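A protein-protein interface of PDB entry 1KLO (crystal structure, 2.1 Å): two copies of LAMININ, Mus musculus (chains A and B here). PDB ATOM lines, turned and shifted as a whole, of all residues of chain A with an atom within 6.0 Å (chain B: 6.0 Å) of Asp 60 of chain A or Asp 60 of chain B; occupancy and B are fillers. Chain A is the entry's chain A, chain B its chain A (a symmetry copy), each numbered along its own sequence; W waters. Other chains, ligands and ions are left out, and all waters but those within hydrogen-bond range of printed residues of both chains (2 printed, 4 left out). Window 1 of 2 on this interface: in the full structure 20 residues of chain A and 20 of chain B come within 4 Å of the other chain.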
ATOM      1  N   PRO A  55      12.561  16.664  13.039  1.00  0.00           N
ATOM      2  CA  PRO A  55      12.206  16.480  11.632  1.00  0.00           C
ATOM      3  C   PRO A  55      11.645  17.774  11.044  1.00  0.00           C
ATOM      4  O   PRO A  55      10.956  18.524  11.738  1.00  0.00           O
ATOM      5  CB  PRO A  55      11.139  15.417  11.702  1.00  0.00           C
ATOM      6  CG  PRO A  55      11.549  14.617  12.889  1.00  0.00           C
ATOM      7  CD  PRO A  55      11.853  15.678  13.872  1.00  0.00           C
ATOM      8  N   CYS A  56      11.950  18.049   9.784  1.00  0.00           N
ATOM      9  CA  CYS A  56      11.424  19.232   9.124  1.00  0.00           C
ATOM     10  C   CYS A  56       9.909  19.310   9.333  1.00  0.00           C
ATOM     11  O   CYS A  56       9.224  18.276   9.344  1.00  0.00           O
ATOM     12  CB  CYS A  56      11.630  19.145   7.635  1.00  0.00           C
ATOM     13  SG  CYS A  56      13.324  18.956   7.095  1.00  0.00           S
ATOM     14  N   GLN A  57       9.387  20.527   9.453  1.00  0.00           N
ATOM     15  CA  GLN A  57       7.963  20.741   9.645  1.00  0.00           C
ATOM     16  C   GLN A  57       7.441  21.451   8.406  1.00  0.00           C
ATOM     17  O   GLN A  57       7.405  22.676   8.351  1.00  0.00           O
ATOM     18  CB  GLN A  57       7.746  21.542  10.935  1.00  0.00           C
ATOM     19  CG  GLN A  57       8.279  20.757  12.114  1.00  0.00           C
ATOM     20  CD  GLN A  57       8.230  21.438  13.458  1.00  0.00           C
ATOM     21  OE1 GLN A  57       7.983  20.775  14.458  1.00  0.00           O
ATOM     22  NE2 GLN A  57       8.511  22.734  13.511  1.00  0.00           N
ATOM     23  N   CYS A  58       7.064  20.660   7.401  1.00  0.00           N
ATOM     24  CA  CYS A  58       6.598  21.190   6.137  1.00  0.00           C
ATOM     25  C   CYS A  58       5.191  20.797   5.763  1.00  0.00           C
ATOM     26  O   CYS A  58       4.891  20.566   4.593  1.00  0.00           O
ATOM     27  CB  CYS A  58       7.551  20.764   5.046  1.00  0.00           C
ATOM     28  SG  CYS A  58       9.233  21.331   5.413  1.00  0.00           S
ATOM     29  N   ASN A  59       4.332  20.709   6.770  1.00  0.00           N
ATOM     30  CA  ASN A  59       2.926  20.366   6.592  1.00  0.00           C
ATOM     31  C   ASN A  59       2.688  19.168   5.716  1.00  0.00           C
ATOM     32  O   ASN A  59       1.717  19.127   4.985  1.00  0.00           O
ATOM     33  CB  ASN A  59       2.158  21.565   6.049  1.00  0.00           C
ATOM     34  CG  ASN A  59       2.041  22.687   7.073  1.00  0.00           C
ATOM     35  OD1 ASN A  59       1.308  22.566   8.048  1.00  0.00           O
ATOM     36  ND2 ASN A  59       2.785  23.759   6.872  1.00  0.00           N
ATOM     37  N   ASP A  60       3.583  18.189   5.819  1.00  0.00           N
ATOM     38  CA  ASP A  60       3.534  16.937   5.063  1.00  0.00           C
ATOM     39  C   ASP A  60       3.459  17.119   3.547  1.00  0.00           C
ATOM     40  O   ASP A  60       2.960  16.255   2.827  1.00  0.00           O
ATOM     41  CB  ASP A  60       2.374  16.088   5.554  1.00  0.00           C
ATOM     42  CG  ASP A  60       2.435  15.846   7.030  1.00  0.00           C
ATOM     43  OD1 ASP A  60       3.517  15.493   7.529  1.00  0.00           O
ATOM     44  OD2 ASP A  60       1.398  16.007   7.697  1.00  0.00           O
ATOM     45  N   ASN A  61       3.967  18.247   3.070  1.00  0.00           N
ATOM     46  CA  ASN A  61       3.957  18.530   1.659  1.00  0.00           C
ATOM     47  C   ASN A  61       5.356  18.419   1.061  1.00  0.00           C
ATOM     48  O   ASN A  61       5.722  19.203   0.196  1.00  0.00           O
ATOM     49  CB  ASN A  61       3.381  19.930   1.410  1.00  0.00           C
ATOM     50  CG  ASN A  61       1.876  20.001   1.646  1.00  0.00           C
ATOM     51  OD1 ASN A  61       1.162  19.022   1.484  1.00  0.00           O
ATOM     52  ND2 ASN A  61       1.394  21.170   2.028  1.00  0.00           N
ATOM     53  N   ILE A  62       6.140  17.457   1.551  1.00  0.00           N
ATOM     54  CA  ILE A  62       7.501  17.185   1.053  1.00  0.00           C
ATOM     55  C   ILE A  62       7.645  15.673   0.848  1.00  0.00           C
ATOM     56  O   ILE A  62       7.039  14.879   1.573  1.00  0.00           O
ATOM     57  CB  ILE A  62       8.651  17.654   2.027  1.00  0.00           C
ATOM     58  CG1 ILE A  62       8.408  17.134   3.443  1.00  0.00           C
ATOM     59  CG2 ILE A  62       8.834  19.141   1.934  1.00  0.00           C
ATOM     60  CD1 ILE A  62       9.551  17.342   4.372  1.00  0.00           C
ATOM     61  N   ILE A  81       6.136  19.994  -2.473  1.00  0.00           N
ATOM     62  CA  ILE A  81       5.527  19.339  -3.631  1.00  0.00           C
ATOM     63  C   ILE A  81       4.048  19.663  -3.738  1.00  0.00           C
ATOM     64  O   ILE A  81       3.505  20.360  -2.886  1.00  0.00           O
ATOM     65  CB  ILE A  81       5.708  17.827  -3.580  1.00  0.00           C
ATOM     66  CG1 ILE A  81       5.035  17.231  -2.349  1.00  0.00           C
ATOM     67  CG2 ILE A  81       7.176  17.504  -3.530  1.00  0.00           C
ATOM     68  CD1 ILE A  81       5.118  15.703  -2.302  1.00  0.00           C
ATOM     69  N   TYR A  82       3.404  19.174  -4.795  1.00  0.00           N
ATOM     70  CA  TYR A  82       1.967  19.384  -5.050  1.00  0.00           C
ATOM     71  C   TYR A  82       1.619  20.824  -5.357  1.00  0.00           C
ATOM     72  O   TYR A  82       0.498  21.260  -5.096  1.00  0.00           O
ATOM     73  CB  TYR A  82       1.108  18.924  -3.872  1.00  0.00           C
ATOM     74  CG  TYR A  82       1.290  17.489  -3.506  1.00  0.00           C
ATOM     75  CD1 TYR A  82       1.320  16.514  -4.489  1.00  0.00           C
ATOM     76  CD2 TYR A  82       1.462  17.105  -2.186  1.00  0.00           C
ATOM     77  CE1 TYR A  82       1.519  15.192  -4.180  1.00  0.00           C
ATOM     78  CE2 TYR A  82       1.664  15.786  -1.866  1.00  0.00           C
ATOM     79  CZ  TYR A  82       1.690  14.838  -2.882  1.00  0.00           C
ATOM     80  OH  TYR A  82       1.894  13.518  -2.620  1.00  0.00           O
ATOM     81  N   LYS A 108      -5.093  20.277  -3.171  1.00  0.00           N
ATOM     82  CA  LYS A 108      -4.212  21.274  -2.602  1.00  0.00           C
ATOM     83  C   LYS A 108      -4.104  22.476  -3.481  1.00  0.00           C
ATOM     84  O   LYS A 108      -4.779  23.456  -3.246  1.00  0.00           O
ATOM     85  CB  LYS A 108      -2.836  20.703  -2.317  1.00  0.00           C
ATOM     86  CG  LYS A 108      -2.880  19.585  -1.332  1.00  0.00           C
ATOM     87  CD  LYS A 108      -1.503  19.090  -1.037  1.00  0.00           C
ATOM     88  CE  LYS A 108      -1.522  17.999  -0.012  1.00  0.00           C
ATOM     89  NZ  LYS A 108      -1.514  18.589   1.337  1.00  0.00           N
ATOM     90  N   PRO B  55       2.214  11.568   1.433  1.00  0.00           N
ATOM     91  CA  PRO B  55       3.139  11.295   2.533  1.00  0.00           C
ATOM     92  C   PRO B  55       2.375  11.063   3.836  1.00  0.00           C
ATOM     93  O   PRO B  55       1.342  11.693   4.070  1.00  0.00           O
ATOM     94  CB  PRO B  55       3.944  12.567   2.604  1.00  0.00           C
ATOM     95  CG  PRO B  55       3.960  13.027   1.187  1.00  0.00           C
ATOM     96  CD  PRO B  55       2.542  12.858   0.806  1.00  0.00           C
ATOM     97  N   CYS B  56       2.861  10.154   4.669  1.00  0.00           N
ATOM     98  CA  CYS B  56       2.231   9.898   5.953  1.00  0.00           C
ATOM     99  C   CYS B  56       1.997  11.221   6.688  1.00  0.00           C
ATOM    100  O   CYS B  56       2.825  12.141   6.599  1.00  0.00           O
ATOM    101  CB  CYS B  56       3.141   9.090   6.840  1.00  0.00           C
ATOM    102  SG  CYS B  56       3.657   7.507   6.187  1.00  0.00           S
ATOM    103  N   GLN B  57       0.903  11.299   7.439  1.00  0.00           N
ATOM    104  CA  GLN B  57       0.570  12.494   8.196  1.00  0.00           C
ATOM    105  C   GLN B  57       0.655  12.135   9.671  1.00  0.00           C
ATOM    106  O   GLN B  57      -0.331  11.729  10.277  1.00  0.00           O
ATOM    107  CB  GLN B  57      -0.821  12.982   7.774  1.00  0.00           C
ATOM    108  CG  GLN B  57      -0.810  13.332   6.301  1.00  0.00           C
ATOM    109  CD  GLN B  57      -2.127  13.745   5.694  1.00  0.00           C
ATOM    110  OE1 GLN B  57      -2.143  14.620   4.836  1.00  0.00           O
ATOM    111  NE2 GLN B  57      -3.221  13.100   6.080  1.00  0.00           N
ATOM    112  N   CYS B  58       1.859  12.263  10.229  1.00  0.00           N
ATOM    113  CA  CYS B  58       2.109  11.906  11.610  1.00  0.00           C
ATOM    114  C   CYS B  58       2.595  13.037  12.480  1.00  0.00           C
ATOM    115  O   CYS B  58       3.430  12.840  13.362  1.00  0.00           O
ATOM    116  CB  CYS B  58       3.103  10.770  11.649  1.00  0.00           C
ATOM    117  SG  CYS B  58       2.486   9.350  10.708  1.00  0.00           S
ATOM    118  N   ASN B  59       2.077  14.229  12.216  1.00  0.00           N
ATOM    119  CA  ASN B  59       2.413  15.430  12.972  1.00  0.00           C
ATOM    120  C   ASN B  59       3.886  15.638  13.181  1.00  0.00           C
ATOM    121  O   ASN B  59       4.295  16.129  14.216  1.00  0.00           O
ATOM    122  CB  ASN B  59       1.696  15.422  14.317  1.00  0.00           C
ATOM    123  CG  ASN B  59       0.190  15.600  14.169  1.00  0.00           C
ATOM    124  OD1 ASN B  59      -0.280  16.685  13.842  1.00  0.00           O
ATOM    125  ND2 ASN B  59      -0.562  14.535  14.374  1.00  0.00           N
ATOM    126  N   ASP B  60       4.671  15.270  12.172  1.00  0.00           N
ATOM    127  CA  ASP B  60       6.130  15.392  12.168  1.00  0.00           C
ATOM    128  C   ASP B  60       6.822  14.715  13.350  1.00  0.00           C
ATOM    129  O   ASP B  60       7.923  15.096  13.746  1.00  0.00           O
ATOM    130  CB  ASP B  60       6.519  16.859  12.092  1.00  0.00           C
ATOM    131  CG  ASP B  60       5.898  17.549  10.918  1.00  0.00           C
ATOM    132  OD1 ASP B  60       5.950  16.994   9.808  1.00  0.00           O
ATOM    133  OD2 ASP B  60       5.357  18.653  11.102  1.00  0.00           O
ATOM    134  N   ASN B  61       6.170  13.702  13.905  1.00  0.00           N
ATOM    135  CA  ASN B  61       6.723  12.984  15.023  1.00  0.00           C
ATOM    136  C   ASN B  61       7.197  11.594  14.610  1.00  0.00           C
ATOM    137  O   ASN B  61       7.042  10.640  15.362  1.00  0.00           O
ATOM    138  CB  ASN B  61       5.681  12.880  16.145  1.00  0.00           C
ATOM    139  CG  ASN B  61       5.439  14.210  16.852  1.00  0.00           C
ATOM    140  OD1 ASN B  61       6.317  15.058  16.925  1.00  0.00           O
ATOM    141  ND2 ASN B  61       4.240  14.389  17.377  1.00  0.00           N
ATOM    142  N   ILE B  62       7.748  11.486  13.401  1.00  0.00           N
ATOM    143  CA  ILE B  62       8.298  10.226  12.867  1.00  0.00           C
ATOM    144  C   ILE B  62       9.670  10.522  12.253  1.00  0.00           C
ATOM    145  O   ILE B  62       9.903  11.615  11.730  1.00  0.00           O
ATOM    146  CB  ILE B  62       7.405   9.552  11.754  1.00  0.00           C
ATOM    147  CG1 ILE B  62       7.037  10.560  10.667  1.00  0.00           C
ATOM    148  CG2 ILE B  62       6.230   8.859  12.383  1.00  0.00           C
ATOM    149  CD1 ILE B  62       6.385   9.959   9.474  1.00  0.00           C
ATOM    150  N   ILE B  81       7.890   8.838  17.350  1.00  0.00           N
ATOM    151  CA  ILE B  81       9.058   9.045  18.205  1.00  0.00           C
ATOM    152  C   ILE B  81       8.799  10.115  19.251  1.00  0.00           C
ATOM    153  O   ILE B  81       7.727  10.712  19.270  1.00  0.00           O
ATOM    154  CB  ILE B  81      10.290   9.425  17.392  1.00  0.00           C
ATOM    155  CG1 ILE B  81      10.074  10.734  16.641  1.00  0.00           C
ATOM    156  CG2 ILE B  81      10.580   8.338  16.394  1.00  0.00           C
ATOM    157  CD1 ILE B  81      11.317  11.198  15.878  1.00  0.00           C
ATOM    158  N   TYR B  82       9.772  10.339  20.130  1.00  0.00           N
ATOM    159  CA  TYR B  82       9.691  11.346  21.204  1.00  0.00           C
ATOM    160  C   TYR B  82       8.656  11.015  22.258  1.00  0.00           C
ATOM    161  O   TYR B  82       8.111  11.914  22.895  1.00  0.00           O
ATOM    162  CB  TYR B  82       9.386  12.740  20.654  1.00  0.00           C
ATOM    163  CG  TYR B  82      10.377  13.233  19.655  1.00  0.00           C
ATOM    164  CD1 TYR B  82      11.735  13.096  19.890  1.00  0.00           C
ATOM    165  CD2 TYR B  82       9.965  13.810  18.465  1.00  0.00           C
ATOM    166  CE1 TYR B  82      12.666  13.513  18.972  1.00  0.00           C
ATOM    167  CE2 TYR B  82      10.886  14.229  17.539  1.00  0.00           C
ATOM    168  CZ  TYR B  82      12.241  14.071  17.810  1.00  0.00           C
ATOM    169  OH  TYR B  82      13.196  14.461  16.923  1.00  0.00           O
ATOM    170  N   LYS B 108       7.661  17.741  24.231  1.00  0.00           N
ATOM    171  CA  LYS B 108       6.546  16.930  23.788  1.00  0.00           C
ATOM    172  C   LYS B 108       6.044  16.044  24.879  1.00  0.00           C
ATOM    173  O   LYS B 108       5.077  16.381  25.530  1.00  0.00           O
ATOM    174  CB  LYS B 108       6.907  16.108  22.565  1.00  0.00           C
ATOM    175  CG  LYS B 108       7.284  16.960  21.401  1.00  0.00           C
ATOM    176  CD  LYS B 108       7.576  16.117  20.205  1.00  0.00           C
ATOM    177  CE  LYS B 108       7.908  16.958  19.011  1.00  0.00           C
ATOM    178  NZ  LYS B 108       6.666  17.356  18.328  1.00  0.00           N
HETATM  179  O   HOH W   1       0.398  15.463  10.251  1.00  0.00           O
HETATM  180  O   HOH W   2       4.349  20.808   9.632  1.00  0.00           O
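Among the printed residues, pairs that only touch across the chains: Pro 55 of chain A with Asp 60 of chain B (3.8 Å), Pro 55 of chain A with Ile 62 of chain B (3.6 Å), Pro 55 of chain A with Tyr 82 of chain B (3.5 Å), Cys 56 of chain A with Asp 60 of chain B (3.5 Å), Gln 57 of chain A with Asp 60 of chain B (3.6 Å), Asp 60 of chain A with Pro 55 of chain B (3.8 Å), Asp 60 of chain A with Cys 56 of chain B (3.5 Å), Asp 60 of chain A with Gln 57 of chain B (3.6 Å), Asp 60 of chain A with Asp 60 of chain B (3.7 Å), Ile 62 of chain A with Pro 55 of chain B (3.6 Å) and Tyr 82 of chain A with Pro 55 of chain B (3.5 Å).
Printed residues of chain B within 4 Å of Pro 55 of chain A: Asp 60 (3.8 Å), Ile 62 (3.6 Å) and Tyr 82 (3.5 Å). Printed residues of chain B within 4 Å of Cys 56 of chain A: Asp 60 (3.5 Å). Of chain B, only Pro 55 (3.8 Å), Cys 56 (3.5 Å), Gln 57 (3.6 Å) and Asp 60 (3.7 Å) come within 4 Å of Asp 60 of chain A. Of the printed residues of chain A, Cys 56 of chain B touches Asp 60. Of the printed residues of chain A, Gln 57 of chain B touches Asp 60. Of chain A, only Pro 55, Cys 56, Gln 57 and Asp 60 come within 4 Å of Asp 60 of chain B. Of the printed residues of chain A, Ile 62 of chain B touches Pro 55. The nearest printed residue of chain B that does not touch Tyr 82 of chain A is Gln 57 of chain B (7.8 Å).
Hydrophobic or aromatic side chains of chain B that line the printed part of chain A: Pro 55 and Tyr 82. Among the printed residues, no Asp or Glu carboxylate lies within 4 Å of a Lys or Arg side-chain nitrogen of the other chain.
Pro 55 of chain A touches Asp 60 of chain B, and with the chains exchanged Asp 60 of chain A touches Pro 55 of chain B. Pro 55 of chain A touches Ile 62 of chain B, and with the chains exchanged Ile 62 of chain A touches Pro 55 of chain B. Pro 55 of chain A touches Tyr 82 of chain B, and with the chains exchanged Tyr 82 of chain A touches Pro 55 of chain B. Cys 56 of chain A touches Asp 60 of chain B, and with the chains exchanged Asp 60 of chain A touches Cys 56 of chain B. 11 positions are printed for both chains. Of the 11 pairs that touch across the chains among the printed residues, 11 have their exchanged pair printed and touching as well.
Water W1 bridges OD2 of Asp 60 of chain A and N of Asn 59 of chain B. Water W2 bridges OD2 of Asp 60 of chain B and N of Asn 59 of chain A.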
